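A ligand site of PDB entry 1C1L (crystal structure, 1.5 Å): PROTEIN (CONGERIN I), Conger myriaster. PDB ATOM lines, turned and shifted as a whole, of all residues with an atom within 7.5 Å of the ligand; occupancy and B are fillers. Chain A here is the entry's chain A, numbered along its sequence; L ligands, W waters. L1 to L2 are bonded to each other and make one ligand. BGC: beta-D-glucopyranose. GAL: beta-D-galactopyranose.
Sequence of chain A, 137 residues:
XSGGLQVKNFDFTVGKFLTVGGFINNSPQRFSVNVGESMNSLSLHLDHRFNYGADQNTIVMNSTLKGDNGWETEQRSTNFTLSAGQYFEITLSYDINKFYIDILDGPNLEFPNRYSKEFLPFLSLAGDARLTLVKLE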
ATOM      1  N   ARG A  30     -20.918  35.798  28.996  1.00  0.00           N
ATOM      2  CA  ARG A  30     -21.261  34.782  28.018  1.00  0.00           C
ATOM      3  C   ARG A  30     -22.403  33.930  28.527  1.00  0.00           C
ATOM      4  O   ARG A  30     -22.677  33.961  29.733  1.00  0.00           O
ATOM      5  CB  ARG A  30     -20.070  33.844  27.763  1.00  0.00           C
ATOM      6  CG  ARG A  30     -19.587  33.100  29.015  1.00  0.00           C
ATOM      7  CD  ARG A  30     -18.344  32.334  28.611  1.00  0.00           C
ATOM      8  NE  ARG A  30     -17.754  31.617  29.725  1.00  0.00           N
ATOM      9  CZ  ARG A  30     -17.406  30.334  29.666  1.00  0.00           C
ATOM     10  NH1 ARG A  30     -17.577  29.584  28.573  1.00  0.00           N
ATOM     11  NH2 ARG A  30     -16.869  29.772  30.741  1.00  0.00           N
ATOM     12  N   SER A  32     -24.384  29.863  27.510  1.00  0.00           N
ATOM     13  CA  SER A  32     -24.469  28.738  26.607  1.00  0.00           C
ATOM     14  C   SER A  32     -25.771  27.960  26.694  1.00  0.00           C
ATOM     15  O   SER A  32     -26.460  27.924  27.711  1.00  0.00           O
ATOM     16  CB  SER A  32     -23.327  27.785  26.884  1.00  0.00           C
ATOM     17  OG  SER A  32     -23.253  27.425  28.260  1.00  0.00           O
ATOM     18  N   ASN A  34     -26.831  24.133  26.196  1.00  0.00           N
ATOM     19  CA  ASN A  34     -26.201  22.832  26.297  1.00  0.00           C
ATOM     20  C   ASN A  34     -27.216  21.723  26.114  1.00  0.00           C
ATOM     21  O   ASN A  34     -28.206  21.703  26.841  1.00  0.00           O
ATOM     22  CB  ASN A  34     -25.562  22.664  27.667  1.00  0.00           C
ATOM     23  CG  ASN A  34     -24.636  23.806  27.987  1.00  0.00           C
ATOM     24  OD1 ASN A  34     -23.476  23.844  27.555  1.00  0.00           O
ATOM     25  ND2 ASN A  34     -25.120  24.834  28.686  1.00  0.00           N
ATOM     26  N   HIS A  45     -22.491  22.292  22.986  1.00  0.00           N
ATOM     27  CA  HIS A  45     -22.328  23.392  23.911  1.00  0.00           C
ATOM     28  C   HIS A  45     -22.244  24.568  22.964  1.00  0.00           C
ATOM     29  O   HIS A  45     -21.301  24.628  22.173  1.00  0.00           O
ATOM     30  CB  HIS A  45     -21.036  23.254  24.699  1.00  0.00           C
ATOM     31  CG  HIS A  45     -20.596  24.481  25.496  1.00  0.00           C
ATOM     32  ND1 HIS A  45     -21.072  24.957  26.627  1.00  0.00           N
ATOM     33  CD2 HIS A  45     -19.518  25.259  25.158  1.00  0.00           C
ATOM     34  CE1 HIS A  45     -20.343  25.982  26.993  1.00  0.00           C
ATOM     35  NE2 HIS A  45     -19.417  26.157  26.095  1.00  0.00           N
ATOM     36  N   LEU A  46     -23.190  25.499  22.984  1.00  0.00           N
ATOM     37  CA  LEU A  46     -23.224  26.632  22.078  1.00  0.00           C
ATOM     38  C   LEU A  46     -23.042  27.855  22.940  1.00  0.00           C
ATOM     39  O   LEU A  46     -23.966  28.277  23.648  1.00  0.00           O
ATOM     40  CB  LEU A  46     -24.571  26.657  21.354  1.00  0.00           C
ATOM     41  CG  LEU A  46     -24.885  27.896  20.504  1.00  0.00           C
ATOM     42  CD1 LEU A  46     -23.975  27.956  19.300  1.00  0.00           C
ATOM     43  CD2 LEU A  46     -26.335  27.866  20.088  1.00  0.00           C
ATOM     44  N   ASP A  47     -21.838  28.430  22.911  1.00  0.00           N
ATOM     45  CA  ASP A  47     -21.478  29.532  23.790  1.00  0.00           C
ATOM     46  C   ASP A  47     -21.413  30.875  23.057  1.00  0.00           C
ATOM     47  O   ASP A  47     -20.682  31.016  22.073  1.00  0.00           O
ATOM     48  CB  ASP A  47     -20.129  29.183  24.430  1.00  0.00           C
ATOM     49  CG  ASP A  47     -19.831  29.887  25.736  1.00  0.00           C
ATOM     50  OD1 ASP A  47     -20.730  30.306  26.459  1.00  0.00           O
ATOM     51  OD2 ASP A  47     -18.661  30.013  26.049  1.00  0.00           O
ATOM     52  N   ARG A  49     -20.180  34.377  23.460  1.00  0.00           N
ATOM     53  CA  ARG A  49     -19.271  35.127  24.300  1.00  0.00           C
ATOM     54  C   ARG A  49     -19.276  36.587  23.878  1.00  0.00           C
ATOM     55  O   ARG A  49     -18.868  36.953  22.768  1.00  0.00           O
ATOM     56  CB  ARG A  49     -17.854  34.561  24.174  1.00  0.00           C
ATOM     57  CG  ARG A  49     -17.778  33.098  24.557  1.00  0.00           C
ATOM     58  CD  ARG A  49     -16.373  32.576  24.390  1.00  0.00           C
ATOM     59  NE  ARG A  49     -16.332  31.247  24.947  1.00  0.00           N
ATOM     60  CZ  ARG A  49     -15.272  30.467  25.055  1.00  0.00           C
ATOM     61  NH1 ARG A  49     -14.088  30.863  24.605  1.00  0.00           N
ATOM     62  NH2 ARG A  49     -15.396  29.260  25.607  1.00  0.00           N
ATOM     63  N   TYR A  52     -15.511  38.402  26.917  1.00  0.00           N
ATOM     64  CA  TYR A  52     -14.872  37.322  27.611  1.00  0.00           C
ATOM     65  C   TYR A  52     -13.407  37.323  27.235  1.00  0.00           C
ATOM     66  O   TYR A  52     -12.918  36.504  26.456  1.00  0.00           O
ATOM     67  CB  TYR A  52     -15.593  36.032  27.208  1.00  0.00           C
ATOM     68  CG  TYR A  52     -15.108  34.820  27.972  1.00  0.00           C
ATOM     69  CD1 TYR A  52     -15.355  34.738  29.343  1.00  0.00           C
ATOM     70  CD2 TYR A  52     -14.452  33.786  27.313  1.00  0.00           C
ATOM     71  CE1 TYR A  52     -14.948  33.622  30.054  1.00  0.00           C
ATOM     72  CE2 TYR A  52     -14.022  32.664  28.018  1.00  0.00           C
ATOM     73  CZ  TYR A  52     -14.287  32.599  29.389  1.00  0.00           C
ATOM     74  OH  TYR A  52     -13.929  31.473  30.103  1.00  0.00           O
ATOM     75  N   ASP A  55     -11.999  36.845  23.672  1.00  0.00           N
ATOM     76  CA  ASP A  55     -13.199  36.578  22.903  1.00  0.00           C
ATOM     77  C   ASP A  55     -14.212  37.662  23.130  1.00  0.00           C
ATOM     78  O   ASP A  55     -14.731  37.868  24.235  1.00  0.00           O
ATOM     79  CB  ASP A  55     -13.770  35.240  23.327  1.00  0.00           C
ATOM     80  CG  ASP A  55     -12.914  34.095  22.844  1.00  0.00           C
ATOM     81  OD1 ASP A  55     -12.294  34.206  21.776  1.00  0.00           O
ATOM     82  OD2 ASP A  55     -12.856  33.091  23.532  1.00  0.00           O
ATOM     83  N   VAL A  60     -18.719  30.071  20.197  1.00  0.00           N
ATOM     84  CA  VAL A  60     -17.859  28.916  20.331  1.00  0.00           C
ATOM     85  C   VAL A  60     -18.772  27.707  20.475  1.00  0.00           C
ATOM     86  O   VAL A  60     -19.657  27.694  21.335  1.00  0.00           O
ATOM     87  CB  VAL A  60     -16.960  29.038  21.578  1.00  0.00           C
ATOM     88  CG1 VAL A  60     -16.135  27.766  21.758  1.00  0.00           C
ATOM     89  CG2 VAL A  60     -16.020  30.233  21.433  1.00  0.00           C
ATOM     90  N   MET A  61     -18.547  26.691  19.668  1.00  0.00           N
ATOM     91  CA  MET A  61     -19.287  25.442  19.720  1.00  0.00           C
ATOM     92  C   MET A  61     -18.316  24.324  20.028  1.00  0.00           C
ATOM     93  O   MET A  61     -17.190  24.273  19.506  1.00  0.00           O
ATOM     94  CB  MET A  61     -19.949  25.170  18.382  1.00  0.00           C
ATOM     95  CG  MET A  61     -21.026  26.194  18.067  1.00  0.00           C
ATOM     96  SD  MET A  61     -21.723  25.920  16.434  1.00  0.00           S
ATOM     97  CE  MET A  61     -20.542  26.856  15.489  1.00  0.00           C
ATOM     98  N   ASN A  62     -18.751  23.414  20.893  1.00  0.00           N
ATOM     99  CA  ASN A  62     -17.920  22.288  21.253  1.00  0.00           C
ATOM    100  C   ASN A  62     -18.809  21.209  21.860  1.00  0.00           C
ATOM    101  O   ASN A  62     -20.033  21.391  21.942  1.00  0.00           O
ATOM    102  CB  ASN A  62     -16.875  22.753  22.266  1.00  0.00           C
ATOM    103  CG  ASN A  62     -15.605  21.923  22.220  1.00  0.00           C
ATOM    104  OD1 ASN A  62     -15.547  20.838  21.630  1.00  0.00           O
ATOM    105  ND2 ASN A  62     -14.549  22.375  22.866  1.00  0.00           N
ATOM    106  N   SER A  63     -18.203  20.106  22.284  1.00  0.00           N
ATOM    107  CA  SER A  63     -18.835  19.009  22.967  1.00  0.00           C
ATOM    108  C   SER A  63     -17.845  18.497  24.021  1.00  0.00           C
ATOM    109  O   SER A  63     -16.676  18.911  24.065  1.00  0.00           O
ATOM    110  CB  SER A  63     -19.145  17.916  21.945  1.00  0.00           C
ATOM    111  OG  SER A  63     -17.973  17.374  21.363  1.00  0.00           O
ATOM    112  N   ASP A  68     -16.077  19.602  32.245  1.00  0.00           N
ATOM    113  CA  ASP A  68     -15.111  20.661  32.008  1.00  0.00           C
ATOM    114  C   ASP A  68     -13.708  20.155  31.668  1.00  0.00           C
ATOM    115  O   ASP A  68     -12.874  20.929  31.209  1.00  0.00           O
ATOM    116  CB  ASP A  68     -15.070  21.553  33.239  1.00  0.00           C
ATOM    117  CG  ASP A  68     -14.449  22.907  32.962  1.00  0.00           C
ATOM    118  OD1 ASP A  68     -14.751  23.532  31.948  1.00  0.00           O
ATOM    119  OD2 ASP A  68     -13.624  23.353  33.771  1.00  0.00           O
ATOM    120  N   ASN A  69     -13.429  18.878  31.869  1.00  0.00           N
ATOM    121  CA  ASN A  69     -12.108  18.376  31.497  1.00  0.00           C
ATOM    122  C   ASN A  69     -12.111  17.609  30.193  1.00  0.00           C
ATOM    123  O   ASN A  69     -11.143  16.920  29.874  1.00  0.00           O
ATOM    124  CB  ASN A  69     -11.546  17.515  32.628  1.00  0.00           C
ATOM    125  CG  ASN A  69     -11.172  18.435  33.772  1.00  0.00           C
ATOM    126  OD1 ASN A  69     -10.422  19.398  33.648  1.00  0.00           O
ATOM    127  ND2 ASN A  69     -11.802  18.268  34.920  1.00  0.00           N
ATOM    128  N   GLY A  70     -13.175  17.682  29.390  1.00  0.00           N
ATOM    129  CA  GLY A  70     -13.180  16.919  28.153  1.00  0.00           C
ATOM    130  C   GLY A  70     -13.497  17.760  26.947  1.00  0.00           C
ATOM    131  O   GLY A  70     -13.881  17.178  25.936  1.00  0.00           O
ATOM    132  N   TRP A  71     -13.433  19.088  26.986  1.00  0.00           N
ATOM    133  CA  TRP A  71     -13.759  19.919  25.832  1.00  0.00           C
ATOM    134  C   TRP A  71     -12.881  19.536  24.662  1.00  0.00           C
ATOM    135  O   TRP A  71     -11.667  19.374  24.837  1.00  0.00           O
ATOM    136  CB  TRP A  71     -13.576  21.390  26.144  1.00  0.00           C
ATOM    137  CG  TRP A  71     -14.502  21.894  27.237  1.00  0.00           C
ATOM    138  CD1 TRP A  71     -14.014  22.337  28.434  1.00  0.00           C
ATOM    139  CD2 TRP A  71     -15.868  21.960  27.168  1.00  0.00           C
ATOM    140  NE1 TRP A  71     -15.068  22.698  29.123  1.00  0.00           N
ATOM    141  CE2 TRP A  71     -16.190  22.504  28.409  1.00  0.00           C
ATOM    142  CE3 TRP A  71     -16.860  21.671  26.228  1.00  0.00           C
ATOM    143  CZ2 TRP A  71     -17.534  22.734  28.735  1.00  0.00           C
ATOM    144  CZ3 TRP A  71     -18.194  21.904  26.552  1.00  0.00           C
ATOM    145  CH2 TRP A  71     -18.535  22.441  27.796  1.00  0.00           C
ATOM    146  N   GLU A  72     -13.497  19.387  23.499  1.00  0.00           N
ATOM    147  CA  GLU A  72     -12.785  18.906  22.342  1.00  0.00           C
ATOM    148  C   GLU A  72     -12.440  20.037  21.370  1.00  0.00           C
ATOM    149  O   GLU A  72     -12.129  21.146  21.819  1.00  0.00           O
ATOM    150  CB  GLU A  72     -13.656  17.829  21.704  1.00  0.00           C
ATOM    151  CG  GLU A  72     -13.986  16.666  22.637  1.00  0.00           C
ATOM    152  CD  GLU A  72     -14.607  15.459  21.968  1.00  0.00           C
ATOM    153  OE1 GLU A  72     -14.529  15.341  20.753  1.00  0.00           O
ATOM    154  OE2 GLU A  72     -15.160  14.620  22.675  1.00  0.00           O
ATOM    155  N   THR A  73     -12.449  19.820  20.047  1.00  0.00           N
ATOM    156  CA  THR A  73     -12.171  20.879  19.091  1.00  0.00           C
ATOM    157  C   THR A  73     -13.285  21.912  18.978  1.00  0.00           C
ATOM    158  O   THR A  73     -14.425  21.621  18.662  1.00  0.00           O
ATOM    159  CB  THR A  73     -11.920  20.234  17.707  1.00  0.00           C
ATOM    160  OG1 THR A  73     -10.855  19.308  17.904  1.00  0.00           O
ATOM    161  CG2 THR A  73     -11.562  21.251  16.607  1.00  0.00           C
ATOM    162  N   GLU A  74     -12.939  23.154  19.289  1.00  0.00           N
ATOM    163  CA  GLU A  74     -13.870  24.255  19.124  1.00  0.00           C
ATOM    164  C   GLU A  74     -14.063  24.606  17.663  1.00  0.00           C
ATOM    165  O   GLU A  74     -13.166  24.485  16.827  1.00  0.00           O
ATOM    166  CB  GLU A  74     -13.351  25.510  19.804  1.00  0.00           C
ATOM    167  CG  GLU A  74     -13.187  25.304  21.292  1.00  0.00           C
ATOM    168  CD  GLU A  74     -12.751  26.551  22.041  1.00  0.00           C
ATOM    169  OE1 GLU A  74     -12.211  27.470  21.448  1.00  0.00           O
ATOM    170  OE2 GLU A  74     -12.966  26.595  23.243  1.00  0.00           O
ATOM    171  N   GLN A  75     -15.315  24.948  17.340  1.00  0.00           N
ATOM    172  CA  GLN A  75     -15.644  25.574  16.088  1.00  0.00           C
ATOM    173  C   GLN A  75     -16.187  26.929  16.524  1.00  0.00           C
ATOM    174  O   GLN A  75     -16.957  27.073  17.460  1.00  0.00           O
ATOM    175  CB  GLN A  75     -16.693  24.770  15.329  1.00  0.00           C
ATOM    176  CG  GLN A  75     -16.065  23.460  14.860  1.00  0.00           C
ATOM    177  CD  GLN A  75     -16.826  22.793  13.721  1.00  0.00           C
ATOM    178  OE1 GLN A  75     -17.623  23.448  13.063  1.00  0.00           O
ATOM    179  NE2 GLN A  75     -16.574  21.540  13.402  1.00  0.00           N
ATOM    180  N   ARG A  76     -15.657  27.982  15.907  1.00  0.00           N
ATOM    181  CA  ARG A  76     -15.956  29.363  16.240  1.00  0.00           C
ATOM    182  C   ARG A  76     -16.588  30.089  15.092  1.00  0.00           C
ATOM    183  O   ARG A  76     -16.364  29.748  13.920  1.00  0.00           O
ATOM    184  CB  ARG A  76     -14.695  30.107  16.628  1.00  0.00           C
ATOM    185  CG  ARG A  76     -14.147  29.580  17.929  1.00  0.00           C
ATOM    186  CD  ARG A  76     -12.744  30.072  18.199  1.00  0.00           C
ATOM    187  NE  ARG A  76     -12.397  29.731  19.560  1.00  0.00           N
ATOM    188  CZ  ARG A  76     -12.317  30.679  20.490  1.00  0.00           C
ATOM    189  NH1 ARG A  76     -12.545  31.943  20.171  1.00  0.00           N
ATOM    190  NH2 ARG A  76     -12.060  30.363  21.758  1.00  0.00           N
HETATM  191  C2  BGC L   1     -10.021  28.030  24.576  1.00  0.00           C
HETATM  192  C3  BGC L   1     -11.218  28.421  25.460  1.00  0.00           C
HETATM  193  C4  BGC L   1     -11.552  27.271  26.396  1.00  0.00           C
HETATM  194  C5  BGC L   1     -10.305  26.890  27.201  1.00  0.00           C
HETATM  195  C6  BGC L   1     -10.546  25.735  28.159  1.00  0.00           C
HETATM  196  C1  BGC L   1      -8.844  27.566  25.426  1.00  0.00           C
HETATM  197  O1  BGC L   1      -7.851  27.092  24.625  1.00  0.00           O
HETATM  198  O2  BGC L   1      -9.640  29.151  23.801  1.00  0.00           O
HETATM  199  O3  BGC L   1     -12.336  28.717  24.646  1.00  0.00           O
HETATM  200  O4  BGC L   1     -12.612  27.685  27.311  1.00  0.00           O
HETATM  201  O5  BGC L   1      -9.272  26.490  26.287  1.00  0.00           O
HETATM  202  O6  BGC L   1     -10.971  24.569  27.467  1.00  0.00           O
HETATM  203  C1  GAL L   2     -13.606  26.765  27.566  1.00  0.00           C
HETATM  204  C2  GAL L   2     -14.560  27.304  28.635  1.00  0.00           C
HETATM  205  C3  GAL L   2     -15.751  26.360  28.820  1.00  0.00           C
HETATM  206  C4  GAL L   2     -16.416  26.062  27.463  1.00  0.00           C
HETATM  207  C5  GAL L   2     -15.367  25.609  26.454  1.00  0.00           C
HETATM  208  C6  GAL L   2     -15.947  25.390  25.078  1.00  0.00           C
HETATM  209  O2  GAL L   2     -13.847  27.423  29.859  1.00  0.00           O
HETATM  210  O3  GAL L   2     -16.675  26.969  29.697  1.00  0.00           O
HETATM  211  O4  GAL L   2     -17.065  27.237  27.003  1.00  0.00           O
HETATM  212  O5  GAL L   2     -14.306  26.583  26.335  1.00  0.00           O
HETATM  213  O6  GAL L   2     -14.967  24.913  24.184  1.00  0.00           O
HETATM  214  O   HOH W   1     -12.282  24.206  24.623  1.00  0.00           O
HETATM  215  O   HOH W   2     -16.769  25.305  31.786  1.00  0.00           O
HETATM  216  O   HOH W   3      -9.653  22.140  26.898  1.00  0.00           O
HETATM  217  O   HOH W   4     -19.521  27.164  30.217  1.00  0.00           O
HETATM  218  O   HOH W   5     -12.676  25.236  31.245  1.00  0.00           O
HETATM  219  O   HOH W   6     -12.306  29.577  29.395  1.00  0.00           O
HETATM  220  O   HOH W   7      -7.337  24.365  27.796  1.00  0.00           O
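An oxygen (O3) of BGC L1 sits at hydrogen-bond distance from the side-chain carboxylate (OE2) of Glu 74 (2.6 Å).
A ring nitrogen (NE2) of His 45 sits at hydrogen-bond distance from an oxygen (O4) of GAL L2.
NH1 of Arg 49 is in hydrogen-bond range of O3 of BGC L1 (2.8 Å).
An oxygen (O4) of GAL L2 is in hydrogen-bond range of the guanidinium group (NH1) of Arg 30 (2.9 Å).
ND2 of Asn 62 sits at hydrogen-bond distance from O6 of GAL L2, at 2.9 Å.
The guanidinium group of Arg 76 lies within hydrogen-bond range of an oxygen (O3) of BGC L1 (3.3 Å).
The side-chain carboxylate of Asp 47 lies within hydrogen-bond range of an oxygen (O4) of GAL L2, at 3.3 Å.
OE1 of Glu 74 lies within salt-bridge range of NH2 of Arg 76, at 2.9 Å.
N of His 45 sits at hydrogen-bond distance from O of Asn 62 (2.8 Å).
ND1 of His 45 sits at hydrogen-bond distance from OD1 of Asn 34, at 2.8 Å.
The guanidinium group (NH1) of Arg 30 is in salt-bridge range of the side-chain carboxylate (OD2) of Asp 47 (2.8 Å).
OH of Tyr 52 lies within hydrogen-bond range of NH2 of Arg 30 (3.5 Å).
The backbone carbonyl oxygen (O) of Thr 73 sits close to the side-chain amide oxygen (OD1) of Asn 62 (3.3 Å).
The guanidinium group (NH1) of Arg 76 is in salt-bridge range of the side-chain carboxylate (OD1) of Asp 55.
The backbone NH (N) of Asp 47 is in hydrogen-bond range of the backbone carbonyl oxygen (O) of Val 60 (2.8 Å).
CG1 of Val 60 touches O6 of GAL L2 (3.9 Å).
CE2 of Trp 71 touches C4 of GAL L2, at 3.7 Å.
Of the 22 residues printed, 9 come within 4 Å of the ligand.
Water W2 lies within hydrogen-bond range of O3 of GAL L2 (2.7 Å) and OD1 of Asp 68 (2.7 Å).
Water W6 lies within hydrogen-bond range of OH of Tyr 52 (2.6 Å) and O2 of GAL L2 (2.7 Å).
Water W1 lies within hydrogen-bond range of an oxygen (O6) of GAL L2 (2.8 Å), the side-chain carboxylate of Glu 74 (2.8 Å) and the side-chain amide nitrogen of Asn 62 (3.4 Å).
Water W5 lies within hydrogen-bond range of OD1 of Asp 68 (2.8 Å) and O2 of GAL L2 (2.8 Å).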
